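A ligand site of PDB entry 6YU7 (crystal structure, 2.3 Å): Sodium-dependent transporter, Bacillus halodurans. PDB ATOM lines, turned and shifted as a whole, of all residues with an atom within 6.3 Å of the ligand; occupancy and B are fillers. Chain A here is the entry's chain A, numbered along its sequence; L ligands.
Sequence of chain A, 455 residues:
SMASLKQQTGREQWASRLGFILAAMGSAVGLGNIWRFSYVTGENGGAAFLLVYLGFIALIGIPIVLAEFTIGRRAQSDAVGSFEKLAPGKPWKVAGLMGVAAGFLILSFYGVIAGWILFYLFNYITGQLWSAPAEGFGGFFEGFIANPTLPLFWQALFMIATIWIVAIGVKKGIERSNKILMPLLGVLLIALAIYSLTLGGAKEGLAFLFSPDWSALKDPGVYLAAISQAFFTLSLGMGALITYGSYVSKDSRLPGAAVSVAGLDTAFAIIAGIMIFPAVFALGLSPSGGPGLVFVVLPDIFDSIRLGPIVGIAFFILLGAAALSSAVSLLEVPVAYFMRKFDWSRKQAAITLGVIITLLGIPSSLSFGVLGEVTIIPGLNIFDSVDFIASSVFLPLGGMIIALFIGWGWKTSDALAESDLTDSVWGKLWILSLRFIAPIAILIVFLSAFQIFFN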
ATOM      1  N   SER A  27       6.471   1.842  22.085  1.00  0.00           N
ATOM      2  CA  SER A  27       5.994   1.753  20.705  1.00  0.00           C
ATOM      3  C   SER A  27       6.283   0.376  20.126  1.00  0.00           C
ATOM      4  O   SER A  27       5.437  -0.204  19.432  1.00  0.00           O
ATOM      5  CB  SER A  27       6.646   2.836  19.854  1.00  0.00           C
ATOM      6  OG  SER A  27       6.355   2.664  18.480  1.00  0.00           O
ATOM      7  N   ALA A  28       7.468  -0.169  20.391  1.00  0.00           N
ATOM      8  CA  ALA A  28       7.885  -1.405  19.734  1.00  0.00           C
ATOM      9  C   ALA A  28       7.196  -2.610  20.348  1.00  0.00           C
ATOM     10  O   ALA A  28       6.639  -3.455  19.630  1.00  0.00           O
ATOM     11  CB  ALA A  28       9.408  -1.551  19.818  1.00  0.00           C
ATOM     12  N   VAL A  29       7.226  -2.733  21.675  1.00  0.00           N
ATOM     13  CA  VAL A  29       6.694  -3.915  22.345  1.00  0.00           C
ATOM     14  C   VAL A  29       5.180  -3.834  22.395  1.00  0.00           C
ATOM     15  O   VAL A  29       4.603  -2.942  23.036  1.00  0.00           O
ATOM     16  CB  VAL A  29       7.287  -4.049  23.754  1.00  0.00           C
ATOM     17  CG1 VAL A  29       6.664  -5.240  24.477  1.00  0.00           C
ATOM     18  CG2 VAL A  29       8.796  -4.209  23.681  1.00  0.00           C
ATOM     19  N   GLY A  30       4.519  -4.775  21.727  1.00  0.00           N
ATOM     20  CA  GLY A  30       3.066  -4.828  21.714  1.00  0.00           C
ATOM     21  C   GLY A  30       2.517  -6.126  21.167  1.00  0.00           C
ATOM     22  O   GLY A  30       3.060  -7.204  21.428  1.00  0.00           O
ATOM     23  N   LEU A  31       1.436  -6.034  20.391  1.00  0.00           N
ATOM     24  CA  LEU A  31       0.805  -7.236  19.847  1.00  0.00           C
ATOM     25  C   LEU A  31       1.722  -7.968  18.876  1.00  0.00           C
ATOM     26  O   LEU A  31       1.602  -9.180  18.697  1.00  0.00           O
ATOM     27  CB  LEU A  31      -0.513  -6.885  19.152  1.00  0.00           C
ATOM     28  CG  LEU A  31      -1.589  -6.222  20.010  1.00  0.00           C
ATOM     29  CD1 LEU A  31      -2.789  -5.841  19.154  1.00  0.00           C
ATOM     30  CD2 LEU A  31      -2.013  -7.146  21.143  1.00  0.00           C
ATOM     31  N   GLY A  32       2.652  -7.241  18.247  1.00  0.00           N
ATOM     32  CA  GLY A  32       3.524  -7.875  17.271  1.00  0.00           C
ATOM     33  C   GLY A  32       4.488  -8.879  17.881  1.00  0.00           C
ATOM     34  O   GLY A  32       4.902  -9.827  17.216  1.00  0.00           O
ATOM     35  N   ASN A  33       4.868  -8.677  19.149  1.00  0.00           N
ATOM     36  CA  ASN A  33       5.814  -9.584  19.790  1.00  0.00           C
ATOM     37  C   ASN A  33       5.168 -10.908  20.141  1.00  0.00           C
ATOM     38  O   ASN A  33       5.814 -11.966  20.072  1.00  0.00           O
ATOM     39  CB  ASN A  33       6.391  -8.930  21.047  1.00  0.00           C
ATOM     40  CG  ASN A  33       7.067  -7.618  20.758  1.00  0.00           C
ATOM     41  OD1 ASN A  33       6.426  -6.658  20.340  1.00  0.00           O
ATOM     42  ND2 ASN A  33       8.375  -7.557  20.978  1.00  0.00           N
ATOM     43  N   GLY A 103       0.081   4.302   8.889  1.00  0.00           N
ATOM     44  CA  GLY A 103      -0.515   4.494  10.197  1.00  0.00           C
ATOM     45  C   GLY A 103      -2.014   4.265  10.184  1.00  0.00           C
ATOM     46  O   GLY A 103      -2.558   3.595  11.065  1.00  0.00           O
ATOM     47  N   ILE A 106      -2.421   0.261   9.359  1.00  0.00           N
ATOM     48  CA  ILE A 106      -1.977  -0.661  10.400  1.00  0.00           C
ATOM     49  C   ILE A 106      -2.846  -0.525  11.643  1.00  0.00           C
ATOM     50  O   ILE A 106      -3.322  -1.534  12.189  1.00  0.00           O
ATOM     51  CB  ILE A 106      -0.489  -0.437  10.731  1.00  0.00           C
ATOM     52  CG1 ILE A 106       0.382  -0.964   9.592  1.00  0.00           C
ATOM     53  CG2 ILE A 106      -0.120  -1.124  12.028  1.00  0.00           C
ATOM     54  CD1 ILE A 106       1.858  -0.962   9.896  1.00  0.00           C
ATOM     55  N   TYR A 110      -5.044  -3.094  13.857  1.00  0.00           N
ATOM     56  CA  TYR A 110      -4.451  -3.209  15.190  1.00  0.00           C
ATOM     57  C   TYR A 110      -5.503  -3.001  16.270  1.00  0.00           C
ATOM     58  O   TYR A 110      -5.485  -3.694  17.296  1.00  0.00           O
ATOM     59  CB  TYR A 110      -3.316  -2.185  15.333  1.00  0.00           C
ATOM     60  CG  TYR A 110      -2.294  -2.550  16.407  1.00  0.00           C
ATOM     61  CD1 TYR A 110      -2.452  -2.097  17.710  1.00  0.00           C
ATOM     62  CD2 TYR A 110      -1.182  -3.313  16.071  1.00  0.00           C
ATOM     63  CE1 TYR A 110      -1.507  -2.413  18.669  1.00  0.00           C
ATOM     64  CE2 TYR A 110      -0.244  -3.629  17.037  1.00  0.00           C
ATOM     65  CZ  TYR A 110      -0.405  -3.186  18.337  1.00  0.00           C
ATOM     66  OH  TYR A 110       0.547  -3.511  19.315  1.00  0.00           O
ATOM     67  N   GLN A 229       7.744  -8.861   9.381  1.00  0.00           N
ATOM     68  CA  GLN A 229       7.653  -8.954  10.832  1.00  0.00           C
ATOM     69  C   GLN A 229       8.708  -8.068  11.502  1.00  0.00           C
ATOM     70  O   GLN A 229       8.435  -7.432  12.524  1.00  0.00           O
ATOM     71  CB  GLN A 229       7.812 -10.404  11.279  1.00  0.00           C
ATOM     72  CG  GLN A 229       7.805 -10.614  12.779  1.00  0.00           C
ATOM     73  CD  GLN A 229       6.458 -10.306  13.407  1.00  0.00           C
ATOM     74  OE1 GLN A 229       5.422 -10.427  12.758  1.00  0.00           O
ATOM     75  NE2 GLN A 229       6.474  -9.902  14.670  1.00  0.00           N
ATOM     76  N   PHE A 231      10.102  -5.227  10.346  1.00  0.00           N
ATOM     77  CA  PHE A 231       9.654  -3.839  10.280  1.00  0.00           C
ATOM     78  C   PHE A 231       8.449  -3.598  11.181  1.00  0.00           C
ATOM     79  O   PHE A 231       8.364  -2.557  11.855  1.00  0.00           O
ATOM     80  CB  PHE A 231       9.328  -3.452   8.840  1.00  0.00           C
ATOM     81  CG  PHE A 231      10.523  -3.014   8.033  1.00  0.00           C
ATOM     82  CD1 PHE A 231      11.003  -1.715   8.142  1.00  0.00           C
ATOM     83  CD2 PHE A 231      11.157  -3.897   7.166  1.00  0.00           C
ATOM     84  CE1 PHE A 231      12.101  -1.314   7.408  1.00  0.00           C
ATOM     85  CE2 PHE A 231      12.255  -3.496   6.432  1.00  0.00           C
ATOM     86  CZ  PHE A 231      12.728  -2.197   6.548  1.00  0.00           C
ATOM     87  N   PHE A 232       7.508  -4.542  11.207  1.00  0.00           N
ATOM     88  CA  PHE A 232       6.316  -4.390  12.034  1.00  0.00           C
ATOM     89  C   PHE A 232       6.679  -4.309  13.514  1.00  0.00           C
ATOM     90  O   PHE A 232       6.293  -3.356  14.203  1.00  0.00           O
ATOM     91  CB  PHE A 232       5.359  -5.562  11.781  1.00  0.00           C
ATOM     92  CG  PHE A 232       4.024  -5.419  12.472  1.00  0.00           C
ATOM     93  CD1 PHE A 232       3.881  -5.681  13.827  1.00  0.00           C
ATOM     94  CD2 PHE A 232       2.895  -5.049  11.755  1.00  0.00           C
ATOM     95  CE1 PHE A 232       2.658  -5.555  14.455  1.00  0.00           C
ATOM     96  CE2 PHE A 232       1.662  -4.927  12.374  1.00  0.00           C
ATOM     97  CZ  PHE A 232       1.549  -5.189  13.728  1.00  0.00           C
ATOM     98  N   THR A 233       7.423  -5.293  14.018  1.00  0.00           N
ATOM     99  CA  THR A 233       7.688  -5.380  15.442  1.00  0.00           C
ATOM    100  C   THR A 233       8.552  -4.225  15.944  1.00  0.00           C
ATOM    101  O   THR A 233       8.518  -3.920  17.132  1.00  0.00           O
ATOM    102  CB  THR A 233       8.359  -6.715  15.779  1.00  0.00           C
ATOM    103  OG1 THR A 233       8.349  -6.916  17.199  1.00  0.00           O
ATOM    104  CG2 THR A 233       9.800  -6.754  15.277  1.00  0.00           C
ATOM    105  N   LEU A 234       9.320  -3.581  15.067  1.00  0.00           N
ATOM    106  CA  LEU A 234      10.176  -2.469  15.454  1.00  0.00           C
ATOM    107  C   LEU A 234       9.519  -1.115  15.261  1.00  0.00           C
ATOM    108  O   LEU A 234      10.178  -0.086  15.462  1.00  0.00           O
ATOM    109  CB  LEU A 234      11.486  -2.522  14.669  1.00  0.00           C
ATOM    110  CG  LEU A 234      12.386  -3.725  14.974  1.00  0.00           C
ATOM    111  CD1 LEU A 234      13.568  -3.749  14.030  1.00  0.00           C
ATOM    112  CD2 LEU A 234      12.846  -3.697  16.414  1.00  0.00           C
ATOM    113  N   SER A 235       8.237  -1.081  14.888  1.00  0.00           N
ATOM    114  CA  SER A 235       7.532   0.158  14.567  1.00  0.00           C
ATOM    115  C   SER A 235       8.332   0.958  13.546  1.00  0.00           C
ATOM    116  O   SER A 235       8.528   2.174  13.670  1.00  0.00           O
ATOM    117  CB  SER A 235       7.265   0.982  15.832  1.00  0.00           C
ATOM    118  OG  SER A 235       6.572   0.218  16.803  1.00  0.00           O
ATOM    119  N   LEU A 236       8.787   0.260  12.514  1.00  0.00           N
ATOM    120  CA  LEU A 236       9.849   0.739  11.638  1.00  0.00           C
ATOM    121  C   LEU A 236       9.323   1.035  10.244  1.00  0.00           C
ATOM    122  O   LEU A 236       8.368   0.417   9.784  1.00  0.00           O
ATOM    123  CB  LEU A 236      10.978  -0.298  11.558  1.00  0.00           C
ATOM    124  CG  LEU A 236      12.280   0.114  10.867  1.00  0.00           C
ATOM    125  CD1 LEU A 236      12.837   1.352  11.534  1.00  0.00           C
ATOM    126  CD2 LEU A 236      13.285  -1.027  10.910  1.00  0.00           C
ATOM    127  N   MET A 238       7.856   3.654   8.817  1.00  0.00           N
ATOM    128  CA  MET A 238       6.714   4.531   8.560  1.00  0.00           C
ATOM    129  C   MET A 238       6.792   5.838   9.326  1.00  0.00           C
ATOM    130  O   MET A 238       5.785   6.545   9.445  1.00  0.00           O
ATOM    131  CB  MET A 238       5.405   3.805   8.868  1.00  0.00           C
ATOM    132  CG  MET A 238       5.290   3.262  10.278  1.00  0.00           C
ATOM    133  SD  MET A 238       3.582   3.035  10.784  1.00  0.00           S
ATOM    134  CE  MET A 238       3.122   4.725  11.151  1.00  0.00           C
ATOM    135  N   GLY A 239       7.960   6.178   9.867  1.00  0.00           N
ATOM    136  CA  GLY A 239       8.125   7.457  10.535  1.00  0.00           C
ATOM    137  C   GLY A 239       7.592   7.533  11.939  1.00  0.00           C
ATOM    138  O   GLY A 239       7.444   8.638  12.473  1.00  0.00           O
ATOM    139  N   ALA A 240       7.275   6.394  12.557  1.00  0.00           N
ATOM    140  CA  ALA A 240       6.830   6.418  13.953  1.00  0.00           C
ATOM    141  C   ALA A 240       7.971   6.784  14.893  1.00  0.00           C
ATOM    142  O   ALA A 240       7.771   7.514  15.867  1.00  0.00           O
ATOM    143  CB  ALA A 240       6.218   5.071  14.332  1.00  0.00           C
ATOM    144  N   LEU A 241       9.173   6.284  14.612  1.00  0.00           N
ATOM    145  CA  LEU A 241      10.344   6.628  15.406  1.00  0.00           C
ATOM    146  C   LEU A 241      10.939   7.975  15.012  1.00  0.00           C
ATOM    147  O   LEU A 241      11.611   8.602  15.837  1.00  0.00           O
ATOM    148  CB  LEU A 241      11.381   5.523  15.295  1.00  0.00           C
ATOM    149  CG  LEU A 241      10.828   4.126  15.629  1.00  0.00           C
ATOM    150  CD1 LEU A 241      11.934   3.082  15.647  1.00  0.00           C
ATOM    151  CD2 LEU A 241      10.081   4.147  16.967  1.00  0.00           C
ATOM    152  N   ASP A 265      12.796  -5.691  22.322  1.00  0.00           N
ATOM    153  CA  ASP A 265      11.720  -6.204  21.466  1.00  0.00           C
ATOM    154  C   ASP A 265      12.008  -7.639  21.040  1.00  0.00           C
ATOM    155  O   ASP A 265      11.084  -8.464  20.945  1.00  0.00           O
ATOM    156  CB  ASP A 265      11.542  -5.302  20.255  1.00  0.00           C
ATOM    157  CG  ASP A 265      10.283  -5.617  19.469  1.00  0.00           C
ATOM    158  OD1 ASP A 265       9.178  -5.296  19.949  1.00  0.00           O
ATOM    159  OD2 ASP A 265      10.396  -6.198  18.367  1.00  0.00           O
ATOM    160  N   ALA A 322       0.363  -3.075  26.747  1.00  0.00           N
ATOM    161  CA  ALA A 322       1.417  -2.974  25.744  1.00  0.00           C
ATOM    162  C   ALA A 322       0.837  -2.646  24.373  1.00  0.00           C
ATOM    163  O   ALA A 322       1.446  -1.895  23.605  1.00  0.00           O
ATOM    164  CB  ALA A 322       2.219  -4.267  25.697  1.00  0.00           C
ATOM    165  N   SER A 326       1.460   0.897  22.001  1.00  0.00           N
ATOM    166  CA  SER A 326       1.801   0.759  20.587  1.00  0.00           C
ATOM    167  C   SER A 326       0.786   1.468  19.703  1.00  0.00           C
ATOM    168  O   SER A 326       1.154   2.143  18.740  1.00  0.00           O
ATOM    169  CB  SER A 326       1.905  -0.719  20.211  1.00  0.00           C
ATOM    170  OG  SER A 326       2.970  -1.362  20.907  1.00  0.00           O
ATOM    171  N   ALA A 327      -0.502   1.319  20.019  1.00  0.00           N
ATOM    172  CA  ALA A 327      -1.537   2.003  19.247  1.00  0.00           C
ATOM    173  C   ALA A 327      -1.425   3.513  19.362  1.00  0.00           C
ATOM    174  O   ALA A 327      -1.736   4.241  18.406  1.00  0.00           O
ATOM    175  CB  ALA A 327      -2.915   1.545  19.688  1.00  0.00           C
ATOM    176  N   SER A 329       1.373   5.258  19.615  1.00  0.00           N
ATOM    177  CA  SER A 329       2.418   5.681  18.694  1.00  0.00           C
ATOM    178  C   SER A 329       1.975   5.515  17.244  1.00  0.00           C
ATOM    179  O   SER A 329       2.478   6.225  16.358  1.00  0.00           O
ATOM    180  CB  SER A 329       3.704   4.893  18.936  1.00  0.00           C
ATOM    181  OG  SER A 329       3.604   3.571  18.438  1.00  0.00           O
ATOM    182  N   LEU A 330       1.065   4.584  16.970  1.00  0.00           N
ATOM    183  CA  LEU A 330       0.494   4.458  15.625  1.00  0.00           C
ATOM    184  C   LEU A 330      -0.322   5.692  15.276  1.00  0.00           C
ATOM    185  O   LEU A 330      -0.092   6.342  14.246  1.00  0.00           O
ATOM    186  CB  LEU A 330      -0.353   3.195  15.536  1.00  0.00           C
ATOM    187  CG  LEU A 330       0.364   1.927  15.091  1.00  0.00           C
ATOM    188  CD1 LEU A 330      -0.505   0.712  15.342  1.00  0.00           C
ATOM    189  CD2 LEU A 330       0.731   2.031  13.612  1.00  0.00           C
ATOM    190  N   VAL A 333       1.438   9.318  14.410  1.00  0.00           N
ATOM    191  CA  VAL A 333       2.038   9.711  13.136  1.00  0.00           C
ATOM    192  C   VAL A 333       1.045  10.521  12.291  1.00  0.00           C
ATOM    193  O   VAL A 333       1.413  11.597  11.790  1.00  0.00           O
ATOM    194  CB  VAL A 333       2.575   8.490  12.358  1.00  0.00           C
ATOM    195  CG1 VAL A 333       3.017   8.895  10.965  1.00  0.00           C
ATOM    196  CG2 VAL A 333       3.714   7.863  13.118  1.00  0.00           C
ATOM    197  N   LEU A 395       5.910  -0.570   4.773  1.00  0.00           N
ATOM    198  CA  LEU A 395       6.994  -0.561   5.756  1.00  0.00           C
ATOM    199  C   LEU A 395       8.356  -0.878   5.139  1.00  0.00           C
ATOM    200  O   LEU A 395       9.305  -0.118   5.382  1.00  0.00           O
ATOM    201  CB  LEU A 395       6.668  -1.515   6.905  1.00  0.00           C
ATOM    202  CG  LEU A 395       5.461  -1.201   7.797  1.00  0.00           C
ATOM    203  CD1 LEU A 395       5.456  -2.099   9.024  1.00  0.00           C
ATOM    204  CD2 LEU A 395       5.449   0.263   8.210  1.00  0.00           C
HETATM  205  N1  LIG L   1       5.750  -2.502  16.654  1.00  0.00           N
HETATM  206  C1  LIG L   1       4.430  -2.715  17.227  1.00  0.00           C
HETATM  207  C2  LIG L   1       4.290  -4.160  17.710  1.00  0.00           C
HETATM  208  O1  LIG L   1       3.290  -4.507  18.386  1.00  0.00           O
HETATM  209  C3  LIG L   1       3.340  -2.381  16.212  1.00  0.00           C
HETATM  210  C4  LIG L   1       3.594  -1.030  15.543  1.00  0.00           C
HETATM  211  C5  LIG L   1       3.484   0.140  16.285  1.00  0.00           C
HETATM  212  C6  LIG L   1       3.926  -0.966  14.202  1.00  0.00           C
HETATM  213  C7  LIG L   1       3.722   1.362  15.672  1.00  0.00           C
HETATM  214  C8  LIG L   1       4.157   0.256  13.597  1.00  0.00           C
HETATM  215  C9  LIG L   1       4.051   1.418  14.327  1.00  0.00           C
HETATM  216  O2  LIG L   1       4.285   2.654  13.712  1.00  0.00           O
HETATM  217  O3  LIG L   1       5.166  -5.012  17.416  1.00  0.00           O
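The backbone carbonyl oxygen of Phe 232 sits at hydrogen-bond distance from a nitrogen (N1) of the ligand, 2.7 Å away. The backbone NH (N) of Gly 32 is in hydrogen-bond range of an oxygen (O1) of the ligand. A nitrogen (N1) of the ligand lies close to the backbone NH of Ser 235 (3.4 Å). OG of Ser 235 is in hydrogen-bond range of N1 of the ligand. An oxygen (O2) of the ligand lies within hydrogen-bond range of the side-chain sulfur of Met 238. An oxygen (O1) of the ligand lies within hydrogen-bond range of the side-chain hydroxyl (OH) of Tyr 110 (3.1 Å). O of Ala 28 sits close to N1 of the ligand (3.2 Å). The backbone NH (N) of Leu 31 is in hydrogen-bond range of an oxygen (O1) of the ligand, at 3.1 Å. A nitrogen (N1) of the ligand sits at hydrogen-bond distance from the backbone carbonyl oxygen of Thr 233, at 3.1 Å.
The side-chain hydroxyl (OG) of Ser 235 sits at hydrogen-bond distance from the backbone carbonyl oxygen (O) of Ser 27 (2.9 Å). N of Leu 31 sits at hydrogen-bond distance from OH of Tyr 110 (2.9 Å). The backbone carbonyl oxygen of Ala 28 sits close to the side-chain amide oxygen of Asn 33, 3.3 Å away. OG1 of Thr 233 lies within hydrogen-bond range of OD2 of Asp 265, 2.5 Å away. OD1 of Asn 33 lies within hydrogen-bond range of N of Gly 30, 3.0 Å away. The backbone carbonyl oxygen (O) of Ser 326 lies within hydrogen-bond range of the side-chain hydroxyl (OG) of Ser 329 (2.9 Å). The backbone carbonyl oxygen of Val 29 is in hydrogen-bond range of the side-chain hydroxyl of Ser 326, 3.1 Å away. OG of Ser 326 sits at hydrogen-bond distance from O of Ala 322 (3.1 Å).
Ser 27 touches the ligand. C of Gly 30 touches O1 of the ligand, at 3.3 Å. Asn 33 touches the ligand (OD1 to O3, 3.6 Å). CB of Ala 240 touches O2 of the ligand (3.2 Å). O of Ser 326 touches C5 of the ligand, 3.9 Å away. OG of Ser 329 touches C7 of the ligand, 3.5 Å away. Leu 330 touches the ligand. Hydrophobic or aromatic side chains that line the ligand: Tyr 110, Phe 232, Met 238, Ala 240 and Leu 330. The nearest printed residue that does not touch the ligand is Leu 234 (4.1 Å).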
